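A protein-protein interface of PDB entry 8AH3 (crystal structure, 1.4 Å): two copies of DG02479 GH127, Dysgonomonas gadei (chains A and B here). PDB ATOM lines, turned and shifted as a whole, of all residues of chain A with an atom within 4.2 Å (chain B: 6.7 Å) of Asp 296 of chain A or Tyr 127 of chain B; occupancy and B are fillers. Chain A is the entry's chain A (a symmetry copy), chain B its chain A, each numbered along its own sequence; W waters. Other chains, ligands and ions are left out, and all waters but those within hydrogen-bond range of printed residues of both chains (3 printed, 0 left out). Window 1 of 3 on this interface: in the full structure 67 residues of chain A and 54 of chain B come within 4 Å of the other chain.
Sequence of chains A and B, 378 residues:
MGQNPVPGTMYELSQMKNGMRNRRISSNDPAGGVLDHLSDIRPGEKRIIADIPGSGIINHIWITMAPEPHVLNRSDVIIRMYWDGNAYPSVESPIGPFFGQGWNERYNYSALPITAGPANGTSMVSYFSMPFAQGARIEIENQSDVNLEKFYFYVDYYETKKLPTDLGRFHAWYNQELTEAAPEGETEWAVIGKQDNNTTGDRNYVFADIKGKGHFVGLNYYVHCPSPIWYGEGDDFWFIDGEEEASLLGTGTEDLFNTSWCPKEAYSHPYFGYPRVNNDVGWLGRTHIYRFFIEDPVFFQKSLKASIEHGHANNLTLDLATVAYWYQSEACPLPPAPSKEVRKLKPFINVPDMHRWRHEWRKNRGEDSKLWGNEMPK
NE2 of His 60 of chain B sits close to NH2 of Arg 291 of chain A (3.4 Å). The side-chain amide oxygen (OD1) of Asn 22 of chain B lies close to the backbone carbonyl oxygen (O) of Pro 297 of chain A, at 3.4 Å. A ring nitrogen (NE2) of His 60 of chain B is in hydrogen-bond range of the side-chain amide oxygen (OD1) of Asn 258 of chain A. The side-chain hydroxyl (OH) of Tyr 127 of chain B lies within hydrogen-bond range of the side-chain amide nitrogen (ND2) of Asn 258 of chain A (2.8 Å). O of Pro 297 of chain A sits at hydrogen-bond distance from OH of Tyr 158 of chain B (2.7 Å).
Of the 20 printed residues of chain B, 8 touch a printed residue of chain A. Hydrophobic or aromatic side chains of chain B that line the printed part of chain A: Leu 13, His 60, Leu 112, Val 125, Tyr 127 and Tyr 158. Hydrophobic or aromatic side chains of chain A that line the printed part of chain B: Tyr 271, Ile 294, Pro 297 and Val 298. Along chain A the printed residues that touch a printed residue of chain B span positions 258 to 298. Among the printed residues, 15 pairs touch across the chains.
The backbone carbonyl oxygen (O) of Pro 113 of chain B is in hydrogen-bond range of the backbone NH (N) of Tyr 127 of chain B, 2.7 Å away. The backbone carbonyl oxygen of Asp 156 of chain B lies within hydrogen-bond range of the backbone NH of Asn 59 of chain B. OD2 of Asp 296 of chain A lies within salt-bridge range of NH2 of Arg 291 of chain A (2.8 Å). The backbone carbonyl oxygen (O) of Tyr 271 of chain A lies within hydrogen-bond range of the backbone NH (N) of Phe 292 of chain A (2.8 Å). OH of Tyr 271 of chain A lies within hydrogen-bond range of OE2 of Glu 295 of chain A, at 2.6 Å. ND1 of His 60 of chain B is in hydrogen-bond range of OD2 of Asp 156 of chain B, 2.8 Å away.
Among the printed residues, pairs that only touch across the chains: Asn 258 of chain A with Val 125 of chain B (3.7 Å), Tyr 271 of chain A with Leu 112 of chain B (3.9 Å), Tyr 271 of chain A with Tyr 127 of chain B (3.9 Å), Arg 291 of chain A with Tyr 127 of chain B (3.7 Å), Ile 294 of chain A with Leu 13 of chain B (3.5 Å), Asp 296 of chain A with Asn 59 of chain B (3.6 Å), Asp 296 of chain A with His 60 of chain B (3.7 Å), Asp 296 of chain A with Tyr 127 of chain B (3.7 Å), Asp 296 of chain A with Tyr 158 of chain B (3.3 Å) and Val 298 of chain A with Asn 22 of chain B (3.6 Å).
No position is printed for both chains. Of the 15 pairs that touch across the chains among the printed residues, none has its exchanged pair printed and touching as well.
Of chain B, only Asn 59, His 60, Tyr 127 and Tyr 158 come within 4 Å of Asp 296 of chain A. Tyr 127 of chain B touches just these residues of chain A: Asn 258, Tyr 271, Arg 291 and Asp 296. Of the printed residues of chain A, Leu 112 of chain B touches Tyr 271. Of the printed residues of chain A, Val 125 of chain B touches Asn 258 (3.7 Å). Of the printed residues of chain B, Val 298 of chain A touches Asn 22 (3.6 Å). The nearest residue of chain B that does not touch Asp 296 of chain A is Asn 22 of chain B (4.9 Å). The nearest printed residue of chain A that does not touch Tyr 127 of chain B is Glu 295 of chain A (4.4 Å).
Water W1 lies within hydrogen-bond range of the side-chain carboxylate (OD2) of Asp 156 of chain B (2.6 Å), the guanidinium group (NH1) of Arg 291 of chain A (3.0 Å) and a ring nitrogen (ND1) of His 60 of chain B (3.4 Å). Water W3 lies within hydrogen-bond range of OH of Tyr 127 of chain B, O of Phe 292 of chain A, OD1 of Asp 296 of chain A and NE of Arg 291 of chain A. Water W2 lies within hydrogen-bond range of OD2 of Asp 296 of chain A (2.7 Å) and OD1 of Asn 59 of chain B (3.0 Å).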
ATOM      1  N   ASN A 258       7.492   3.976  -6.762  1.00  0.00           N
ATOM      2  CA  ASN A 258       8.894   4.120  -6.403  1.00  0.00           C
ATOM      3  C   ASN A 258       9.337   3.083  -5.343  1.00  0.00           C
ATOM      4  O   ASN A 258      10.275   3.323  -4.614  1.00  0.00           O
ATOM      5  CB  ASN A 258       9.225   5.530  -5.908  1.00  0.00           C
ATOM      6  CG  ASN A 258       9.366   6.552  -7.000  1.00  0.00           C
ATOM      7  OD1 ASN A 258       9.776   6.183  -8.101  1.00  0.00           O
ATOM      8  ND2 ASN A 258       9.131   7.824  -6.674  1.00  0.00           N
ATOM      9  N   TYR A 271       7.804  12.843  -1.552  1.00  0.00           N
ATOM     10  CA  TYR A 271       7.134  12.643  -2.831  1.00  0.00           C
ATOM     11  C   TYR A 271       6.490  11.278  -2.987  1.00  0.00           C
ATOM     12  O   TYR A 271       5.754  11.094  -3.971  1.00  0.00           O
ATOM     13  CB  TYR A 271       8.102  12.845  -4.010  1.00  0.00           C
ATOM     14  CG  TYR A 271       8.723  14.222  -4.070  1.00  0.00           C
ATOM     15  CD1 TYR A 271       8.104  15.320  -3.522  1.00  0.00           C
ATOM     16  CD2 TYR A 271       9.980  14.396  -4.623  1.00  0.00           C
ATOM     17  CE1 TYR A 271       8.673  16.589  -3.619  1.00  0.00           C
ATOM     18  CE2 TYR A 271      10.588  15.643  -4.678  1.00  0.00           C
ATOM     19  CZ  TYR A 271       9.930  16.737  -4.165  1.00  0.00           C
ATOM     20  OH  TYR A 271      10.476  18.018  -4.217  1.00  0.00           O
ATOM     21  N   ARG A 291       2.060   9.048  -4.558  1.00  0.00           N
ATOM     22  CA  ARG A 291       3.190   9.639  -5.249  1.00  0.00           C
ATOM     23  C   ARG A 291       2.764  11.018  -5.761  1.00  0.00           C
ATOM     24  O   ARG A 291       1.687  11.164  -6.326  1.00  0.00           O
ATOM     25  CB  ARG A 291       3.689   8.762  -6.389  1.00  0.00           C
ATOM     26  CG  ARG A 291       4.838   9.387  -7.176  1.00  0.00           C
ATOM     27  CD  ARG A 291       5.486   8.419  -8.128  1.00  0.00           C
ATOM     28  NE  ARG A 291       6.493   9.037  -8.959  1.00  0.00           N
ATOM     29  CZ  ARG A 291       7.011   8.507 -10.065  1.00  0.00           C
ATOM     30  NH1 ARG A 291       6.744   7.255 -10.412  1.00  0.00           N
ATOM     31  NH2 ARG A 291       7.787   9.269 -10.823  1.00  0.00           N
ATOM     32  N   PHE A 292       3.625  11.998  -5.517  1.00  0.00           N
ATOM     33  CA  PHE A 292       3.436  13.353  -6.025  1.00  0.00           C
ATOM     34  C   PHE A 292       4.518  13.619  -7.057  1.00  0.00           C
ATOM     35  O   PHE A 292       5.667  13.217  -6.899  1.00  0.00           O
ATOM     36  CB  PHE A 292       3.451  14.396  -4.904  1.00  0.00           C
ATOM     37  CG  PHE A 292       2.230  14.191  -4.057  1.00  0.00           C
ATOM     38  CD1 PHE A 292       1.006  14.594  -4.548  1.00  0.00           C
ATOM     39  CD2 PHE A 292       2.286  13.617  -2.777  1.00  0.00           C
ATOM     40  CE1 PHE A 292      -0.150  14.359  -3.816  1.00  0.00           C
ATOM     41  CE2 PHE A 292       1.110  13.386  -2.068  1.00  0.00           C
ATOM     42  CZ  PHE A 292      -0.092  13.761  -2.580  1.00  0.00           C
ATOM     43  N   PHE A 293       4.104  14.256  -8.164  1.00  0.00           N
ATOM     44  CA  PHE A 293       4.924  14.494  -9.323  1.00  0.00           C
ATOM     45  C   PHE A 293       5.178  15.996  -9.369  1.00  0.00           C
ATOM     46  O   PHE A 293       4.552  16.746 -10.127  1.00  0.00           O
ATOM     47  CB  PHE A 293       4.232  13.975 -10.594  1.00  0.00           C
ATOM     48  CG  PHE A 293       3.869  12.521 -10.597  1.00  0.00           C
ATOM     49  CD1 PHE A 293       2.723  12.048  -9.953  1.00  0.00           C
ATOM     50  CD2 PHE A 293       4.665  11.597 -11.257  1.00  0.00           C
ATOM     51  CE1 PHE A 293       2.382  10.709  -9.985  1.00  0.00           C
ATOM     52  CE2 PHE A 293       4.319  10.248 -11.280  1.00  0.00           C
ATOM     53  CZ  PHE A 293       3.182   9.807 -10.656  1.00  0.00           C
ATOM     54  N   ILE A 294       6.092  16.398  -8.489  1.00  0.00           N
ATOM     55  CA  ILE A 294       6.370  17.800  -8.237  1.00  0.00           C
ATOM     56  C   ILE A 294       7.578  18.236  -9.062  1.00  0.00           C
ATOM     57  O   ILE A 294       7.529  19.259  -9.774  1.00  0.00           O
ATOM     58  CB  ILE A 294       6.616  18.008  -6.730  1.00  0.00           C
ATOM     59  CG1 ILE A 294       5.457  17.522  -5.842  1.00  0.00           C
ATOM     60  CG2 ILE A 294       6.989  19.440  -6.429  1.00  0.00           C
ATOM     61  CD1 ILE A 294       4.174  18.081  -6.195  1.00  0.00           C
ATOM     62  N   GLU A 295       8.672  17.464  -8.977  1.00  0.00           N
ATOM     63  CA  GLU A 295       9.839  17.712  -9.796  1.00  0.00           C
ATOM     64  C   GLU A 295       9.596  17.202 -11.206  1.00  0.00           C
ATOM     65  O   GLU A 295      10.275  17.647 -12.135  1.00  0.00           O
ATOM     66  CB  GLU A 295      11.066  16.974  -9.253  1.00  0.00           C
ATOM     67  CG  GLU A 295      11.352  17.308  -7.804  1.00  0.00           C
ATOM     68  CD  GLU A 295      11.722  18.737  -7.472  1.00  0.00           C
ATOM     69  OE1 GLU A 295      12.210  19.461  -8.353  1.00  0.00           O
ATOM     70  OE2 GLU A 295      11.523  19.125  -6.304  1.00  0.00           O
ATOM     71  N   ASP A 296       8.675  16.224 -11.333  1.00  0.00           N
ATOM     72  CA  ASP A 296       8.497  15.394 -12.525  1.00  0.00           C
ATOM     73  C   ASP A 296       7.036  15.307 -12.959  1.00  0.00           C
ATOM     74  O   ASP A 296       6.481  14.216 -13.194  1.00  0.00           O
ATOM     75  CB  ASP A 296       9.102  14.001 -12.320  1.00  0.00           C
ATOM     76  CG  ASP A 296       8.470  13.133 -11.245  1.00  0.00           C
ATOM     77  OD1 ASP A 296       7.995  13.731 -10.219  1.00  0.00           O
ATOM     78  OD2 ASP A 296       8.513  11.896 -11.411  1.00  0.00           O
ATOM     79  N   PRO A 297       6.355  16.475 -13.128  1.00  0.00           N
ATOM     80  CA  PRO A 297       4.958  16.438 -13.584  1.00  0.00           C
ATOM     81  C   PRO A 297       4.828  15.824 -14.981  1.00  0.00           C
ATOM     82  O   PRO A 297       5.802  15.800 -15.745  1.00  0.00           O
ATOM     83  CB  PRO A 297       4.563  17.928 -13.561  1.00  0.00           C
ATOM     84  CG  PRO A 297       5.867  18.679 -13.686  1.00  0.00           C
ATOM     85  CD  PRO A 297       6.894  17.832 -12.971  1.00  0.00           C
ATOM     86  N   VAL A 298       3.648  15.267 -15.282  1.00  0.00           N
ATOM     87  CA  VAL A 298       3.397  14.683 -16.593  1.00  0.00           C
ATOM     88  C   VAL A 298       2.602  15.695 -17.408  1.00  0.00           C
ATOM     89  O   VAL A 298       1.419  15.884 -17.157  1.00  0.00           O
ATOM     90  CB  VAL A 298       2.657  13.334 -16.491  1.00  0.00           C
ATOM     91  CG1 VAL A 298       2.441  12.737 -17.879  1.00  0.00           C
ATOM     92  CG2 VAL A 298       3.365  12.353 -15.599  1.00  0.00           C
ATOM     93  N   LEU B  13       4.475  25.123  -9.783  1.00  0.00           N
ATOM     94  CA  LEU B  13       3.780  23.946 -10.259  1.00  0.00           C
ATOM     95  C   LEU B  13       2.408  24.334 -10.812  1.00  0.00           C
ATOM     96  O   LEU B  13       1.808  23.591 -11.597  1.00  0.00           O
ATOM     97  CB  LEU B  13       3.656  22.972  -9.092  1.00  0.00           C
ATOM     98  CG  LEU B  13       3.158  21.586  -9.399  1.00  0.00           C
ATOM     99  CD1 LEU B  13       4.127  20.790 -10.313  1.00  0.00           C
ATOM    100  CD2 LEU B  13       2.976  20.813  -8.107  1.00  0.00           C
ATOM    101  N   ASN B  22       6.671  14.419 -22.158  1.00  0.00           N
ATOM    102  CA  ASN B  22       7.084  13.263 -21.373  1.00  0.00           C
ATOM    103  C   ASN B  22       7.300  12.024 -22.226  1.00  0.00           C
ATOM    104  O   ASN B  22       6.476  11.702 -23.094  1.00  0.00           O
ATOM    105  CB  ASN B  22       6.032  12.885 -20.314  1.00  0.00           C
ATOM    106  CG  ASN B  22       6.055  13.808 -19.132  1.00  0.00           C
ATOM    107  OD1 ASN B  22       6.531  13.426 -18.015  1.00  0.00           O
ATOM    108  ND2 ASN B  22       5.614  15.022 -19.352  1.00  0.00           N
ATOM    109  N   ILE B  58      16.421  13.880 -18.301  1.00  0.00           N
ATOM    110  CA  ILE B  58      15.936  12.837 -17.396  1.00  0.00           C
ATOM    111  C   ILE B  58      15.415  13.500 -16.121  1.00  0.00           C
ATOM    112  O   ILE B  58      16.088  14.354 -15.579  1.00  0.00           O
ATOM    113  CB  ILE B  58      17.038  11.808 -17.108  1.00  0.00           C
ATOM    114  CG1 ILE B  58      17.425  11.089 -18.407  1.00  0.00           C
ATOM    115  CG2 ILE B  58      16.584  10.798 -16.042  1.00  0.00           C
ATOM    116  CD1 ILE B  58      18.621  10.254 -18.327  1.00  0.00           C
ATOM    117  N   ASN B  59      14.209  13.116 -15.689  1.00  0.00           N
ATOM    118  CA  ASN B  59      13.568  13.756 -14.545  1.00  0.00           C
ATOM    119  C   ASN B  59      13.338  12.778 -13.375  1.00  0.00           C
ATOM    120  O   ASN B  59      13.053  13.236 -12.239  1.00  0.00           O
ATOM    121  CB  ASN B  59      12.264  14.409 -14.964  1.00  0.00           C
ATOM    122  CG  ASN B  59      11.224  13.453 -15.512  1.00  0.00           C
ATOM    123  OD1 ASN B  59      10.939  12.418 -14.921  1.00  0.00           O
ATOM    124  ND2 ASN B  59      10.655  13.732 -16.696  1.00  0.00           N
ATOM    125  N   HIS B  60      13.535  11.471 -13.609  1.00  0.00           N
ATOM    126  CA  HIS B  60      13.237  10.462 -12.585  1.00  0.00           C
ATOM    127  C   HIS B  60      13.765   9.133 -13.082  1.00  0.00           C
ATOM    128  O   HIS B  60      13.510   8.747 -14.253  1.00  0.00           O
ATOM    129  CB  HIS B  60      11.743  10.391 -12.340  1.00  0.00           C
ATOM    130  CG  HIS B  60      11.264   9.155 -11.615  1.00  0.00           C
ATOM    131  ND1 HIS B  60      10.721   8.080 -12.296  1.00  0.00           N
ATOM    132  CD2 HIS B  60      11.247   8.840 -10.294  1.00  0.00           C
ATOM    133  CE1 HIS B  60      10.378   7.134 -11.395  1.00  0.00           C
ATOM    134  NE2 HIS B  60      10.706   7.583 -10.159  1.00  0.00           N
ATOM    135  N   ILE B  61      14.454   8.411 -12.192  1.00  0.00           N
ATOM    136  CA  ILE B  61      14.908   7.050 -12.449  1.00  0.00           C
ATOM    137  C   ILE B  61      14.466   6.188 -11.272  1.00  0.00           C
ATOM    138  O   ILE B  61      14.631   6.597 -10.117  1.00  0.00           O
ATOM    139  CB  ILE B  61      16.433   6.960 -12.579  1.00  0.00           C
ATOM    140  CG1 ILE B  61      16.927   7.819 -13.747  1.00  0.00           C
ATOM    141  CG2 ILE B  61      16.953   5.525 -12.678  1.00  0.00           C
ATOM    142  CD1 ILE B  61      18.399   7.990 -13.784  1.00  0.00           C
ATOM    143  N   ALA B 111      16.233  10.523   1.836  1.00  0.00           N
ATOM    144  CA  ALA B 111      16.839  11.765   1.384  1.00  0.00           C
ATOM    145  C   ALA B 111      16.003  12.314   0.230  1.00  0.00           C
ATOM    146  O   ALA B 111      15.323  11.570  -0.470  1.00  0.00           O
ATOM    147  CB  ALA B 111      18.255  11.534   1.000  1.00  0.00           C
ATOM    148  N   LEU B 112      16.091  13.614  -0.042  1.00  0.00           N
ATOM    149  CA  LEU B 112      15.194  14.180  -1.038  1.00  0.00           C
ATOM    150  C   LEU B 112      15.576  13.751  -2.449  1.00  0.00           C
ATOM    151  O   LEU B 112      14.737  13.219  -3.197  1.00  0.00           O
ATOM    152  CB  LEU B 112      15.140  15.713  -0.879  1.00  0.00           C
ATOM    153  CG  LEU B 112      14.200  16.436  -1.839  1.00  0.00           C
ATOM    154  CD1 LEU B 112      12.770  16.086  -1.534  1.00  0.00           C
ATOM    155  CD2 LEU B 112      14.430  17.935  -1.757  1.00  0.00           C
ATOM    156  N   PRO B 113      16.798  14.012  -2.946  1.00  0.00           N
ATOM    157  CA  PRO B 113      17.039  13.825  -4.388  1.00  0.00           C
ATOM    158  C   PRO B 113      17.327  12.412  -4.873  1.00  0.00           C
ATOM    159  O   PRO B 113      17.192  12.105  -6.052  1.00  0.00           O
ATOM    160  CB  PRO B 113      18.310  14.641  -4.664  1.00  0.00           C
ATOM    161  CG  PRO B 113      19.006  14.733  -3.329  1.00  0.00           C
ATOM    162  CD  PRO B 113      17.898  14.698  -2.276  1.00  0.00           C
ATOM    163  N   ILE B 114      17.844  11.571  -3.973  1.00  0.00           N
ATOM    164  CA  ILE B 114      18.227  10.187  -4.240  1.00  0.00           C
ATOM    165  C   ILE B 114      17.834   9.436  -2.985  1.00  0.00           C
ATOM    166  O   ILE B 114      18.097   9.936  -1.897  1.00  0.00           O
ATOM    167  CB  ILE B 114      19.745   9.997  -4.413  1.00  0.00           C
ATOM    168  CG1 ILE B 114      20.215  10.599  -5.712  1.00  0.00           C
ATOM    169  CG2 ILE B 114      20.117   8.495  -4.316  1.00  0.00           C
ATOM    170  CD1 ILE B 114      21.506  10.006  -6.219  1.00  0.00           C
ATOM    171  N   THR B 115      17.216   8.281  -3.126  1.00  0.00           N
ATOM    172  CA  THR B 115      16.874   7.506  -1.941  1.00  0.00           C
ATOM    173  C   THR B 115      16.759   6.025  -2.292  1.00  0.00           C
ATOM    174  O   THR B 115      16.677   5.657  -3.467  1.00  0.00           O
ATOM    175  CB  THR B 115      15.633   8.088  -1.237  1.00  0.00           C
ATOM    176  OG1 THR B 115      15.762   7.788   0.160  1.00  0.00           O
ATOM    177  CG2 THR B 115      14.311   7.614  -1.766  1.00  0.00           C
ATOM    178  N   VAL B 125      15.933   5.104  -6.270  1.00  0.00           N
ATOM    179  CA  VAL B 125      15.204   6.229  -6.835  1.00  0.00           C
ATOM    180  C   VAL B 125      16.119   7.443  -6.955  1.00  0.00           C
ATOM    181  O   VAL B 125      16.800   7.802  -6.015  1.00  0.00           O
ATOM    182  CB  VAL B 125      13.962   6.572  -5.989  1.00  0.00           C
ATOM    183  CG1 VAL B 125      13.211   7.766  -6.564  1.00  0.00           C
ATOM    184  CG2 VAL B 125      13.013   5.387  -5.912  1.00  0.00           C
ATOM    185  N   SER B 126      16.082   8.137  -8.123  1.00  0.00           N
ATOM    186  CA  SER B 126      16.796   9.395  -8.306  1.00  0.00           C
ATOM    187  C   SER B 126      15.826  10.432  -8.897  1.00  0.00           C
ATOM    188  O   SER B 126      15.134  10.119  -9.875  1.00  0.00           O
ATOM    189  CB  SER B 126      18.019   9.261  -9.229  1.00  0.00           C
ATOM    190  OG  SER B 126      18.517  10.561  -9.553  1.00  0.00           O
ATOM    191  N   TYR B 127      15.811  11.630  -8.320  1.00  0.00           N
ATOM    192  CA  TYR B 127      15.124  12.800  -8.855  1.00  0.00           C
ATOM    193  C   TYR B 127      16.095  13.884  -9.359  1.00  0.00           C
ATOM    194  O   TYR B 127      15.663  14.989  -9.702  1.00  0.00           O
ATOM    195  CB  TYR B 127      14.205  13.415  -7.794  1.00  0.00           C
ATOM    196  CG  TYR B 127      12.899  12.670  -7.603  1.00  0.00           C
ATOM    197  CD1 TYR B 127      11.919  12.686  -8.581  1.00  0.00           C
ATOM    198  CD2 TYR B 127      12.730  11.875  -6.484  1.00  0.00           C
ATOM    199  CE1 TYR B 127      10.726  11.982  -8.430  1.00  0.00           C
ATOM    200  CE2 TYR B 127      11.531  11.193  -6.291  1.00  0.00           C
ATOM    201  CZ  TYR B 127      10.550  11.225  -7.279  1.00  0.00           C
ATOM    202  OH  TYR B 127       9.336  10.581  -7.108  1.00  0.00           O
ATOM    203  N   PHE B 128      17.393  13.592  -9.517  1.00  0.00           N
ATOM    204  CA  PHE B 128      18.281  14.533 -10.168  1.00  0.00           C
ATOM    205  C   PHE B 128      17.866  14.737 -11.626  1.00  0.00           C
ATOM    206  O   PHE B 128      17.560  13.774 -12.324  1.00  0.00           O
ATOM    207  CB  PHE B 128      19.721  14.048 -10.103  1.00  0.00           C
ATOM    208  CG  PHE B 128      20.395  14.298  -8.766  1.00  0.00           C
ATOM    209  CD1 PHE B 128      20.636  15.557  -8.323  1.00  0.00           C
ATOM    210  CD2 PHE B 128      20.884  13.229  -8.035  1.00  0.00           C
ATOM    211  CE1 PHE B 128      21.256  15.780  -7.100  1.00  0.00           C
ATOM    212  CE2 PHE B 128      21.595  13.468  -6.867  1.00  0.00           C
ATOM    213  CZ  PHE B 128      21.737  14.726  -6.394  1.00  0.00           C
ATOM    214  N   SER B 129      17.862  15.999 -12.037  1.00  0.00           N
ATOM    215  CA  SER B 129      17.622  16.359 -13.424  1.00  0.00           C
ATOM    216  C   SER B 129      18.913  16.153 -14.234  1.00  0.00           C
ATOM    217  O   SER B 129      19.996  16.566 -13.850  1.00  0.00           O
ATOM    218  CB  SER B 129      17.150  17.810 -13.434  1.00  0.00           C
ATOM    219  OG  SER B 129      17.138  18.365 -14.742  1.00  0.00           O
ATOM    220  N   MET B 130      18.802  15.471 -15.382  1.00  0.00           N
ATOM    221  CA  MET B 130      19.987  15.149 -16.153  1.00  0.00           C
ATOM    222  C   MET B 130      19.768  15.550 -17.614  1.00  0.00           C
ATOM    223  O   MET B 130      19.195  14.769 -18.403  1.00  0.00           O
ATOM    224  CB  MET B 130      20.334  13.671 -16.073  1.00  0.00           C
ATOM    225  CG  MET B 130      20.312  13.125 -14.646  1.00  0.00           C
ATOM    226  SD  MET B 130      20.888  11.429 -14.620  1.00  0.00           S
ATOM    227  CE  MET B 130      20.649  11.032 -12.876  1.00  0.00           C
ATOM    228  N   ASP B 156      12.370   8.102 -16.790  1.00  0.00           N
ATOM    229  CA  ASP B 156      11.423   9.123 -17.186  1.00  0.00           C
ATOM    230  C   ASP B 156      12.182  10.369 -17.625  1.00  0.00           C
ATOM    231  O   ASP B 156      13.142  10.771 -16.996  1.00  0.00           O
ATOM    232  CB  ASP B 156      10.450   9.477 -16.064  1.00  0.00           C
ATOM    233  CG  ASP B 156       9.453   8.368 -15.788  1.00  0.00           C
ATOM    234  OD1 ASP B 156       8.442   8.298 -16.516  1.00  0.00           O
ATOM    235  OD2 ASP B 156       9.674   7.615 -14.801  1.00  0.00           O
ATOM    236  N   TYR B 158      11.956  14.202 -20.243  1.00  0.00           N
ATOM    237  CA  TYR B 158      11.292  15.157 -21.101  1.00  0.00           C
ATOM    238  C   TYR B 158      12.071  15.225 -22.417  1.00  0.00           C
ATOM    239  O   TYR B 158      13.264  15.467 -22.392  1.00  0.00           O
ATOM    240  CB  TYR B 158      11.213  16.550 -20.473  1.00  0.00           C
ATOM    241  CG  TYR B 158      10.448  16.631 -19.172  1.00  0.00           C
ATOM    242  CD1 TYR B 158       9.112  16.293 -19.114  1.00  0.00           C
ATOM    243  CD2 TYR B 158      11.080  17.036 -18.003  1.00  0.00           C
ATOM    244  CE1 TYR B 158       8.407  16.326 -17.930  1.00  0.00           C
ATOM    245  CE2 TYR B 158      10.378  17.087 -16.800  1.00  0.00           C
ATOM    246  CZ  TYR B 158       9.046  16.735 -16.780  1.00  0.00           C
ATOM    247  OH  TYR B 158       8.312  16.783 -15.613  1.00  0.00           O
ATOM    248  N   TYR B 327      27.238  19.019 -11.319  1.00  0.00           N
ATOM    249  CA  TYR B 327      26.953  19.423 -12.690  1.00  0.00           C
ATOM    250  C   TYR B 327      28.164  20.140 -13.294  1.00  0.00           C
ATOM    251  O   TYR B 327      28.885  20.826 -12.597  1.00  0.00           O
ATOM    252  CB  TYR B 327      25.749  20.376 -12.732  1.00  0.00           C
ATOM    253  CG  TYR B 327      24.454  19.655 -12.458  1.00  0.00           C
ATOM    254  CD1 TYR B 327      23.742  19.039 -13.450  1.00  0.00           C
ATOM    255  CD2 TYR B 327      23.985  19.493 -11.143  1.00  0.00           C
ATOM    256  CE1 TYR B 327      22.594  18.295 -13.187  1.00  0.00           C
ATOM    257  CE2 TYR B 327      22.850  18.754 -10.881  1.00  0.00           C
ATOM    258  CZ  TYR B 327      22.158  18.118 -11.881  1.00  0.00           C
ATOM    259  OH  TYR B 327      21.035  17.398 -11.648  1.00  0.00           O
HETATM  260  O   HOH W   1       7.537   7.457 -13.295  1.00  0.00           O
HETATM  261  O   HOH W   2       8.576  10.820 -13.862  1.00  0.00           O
HETATM  262  O   HOH W   3       7.382  11.754  -8.412  1.00  0.00           O
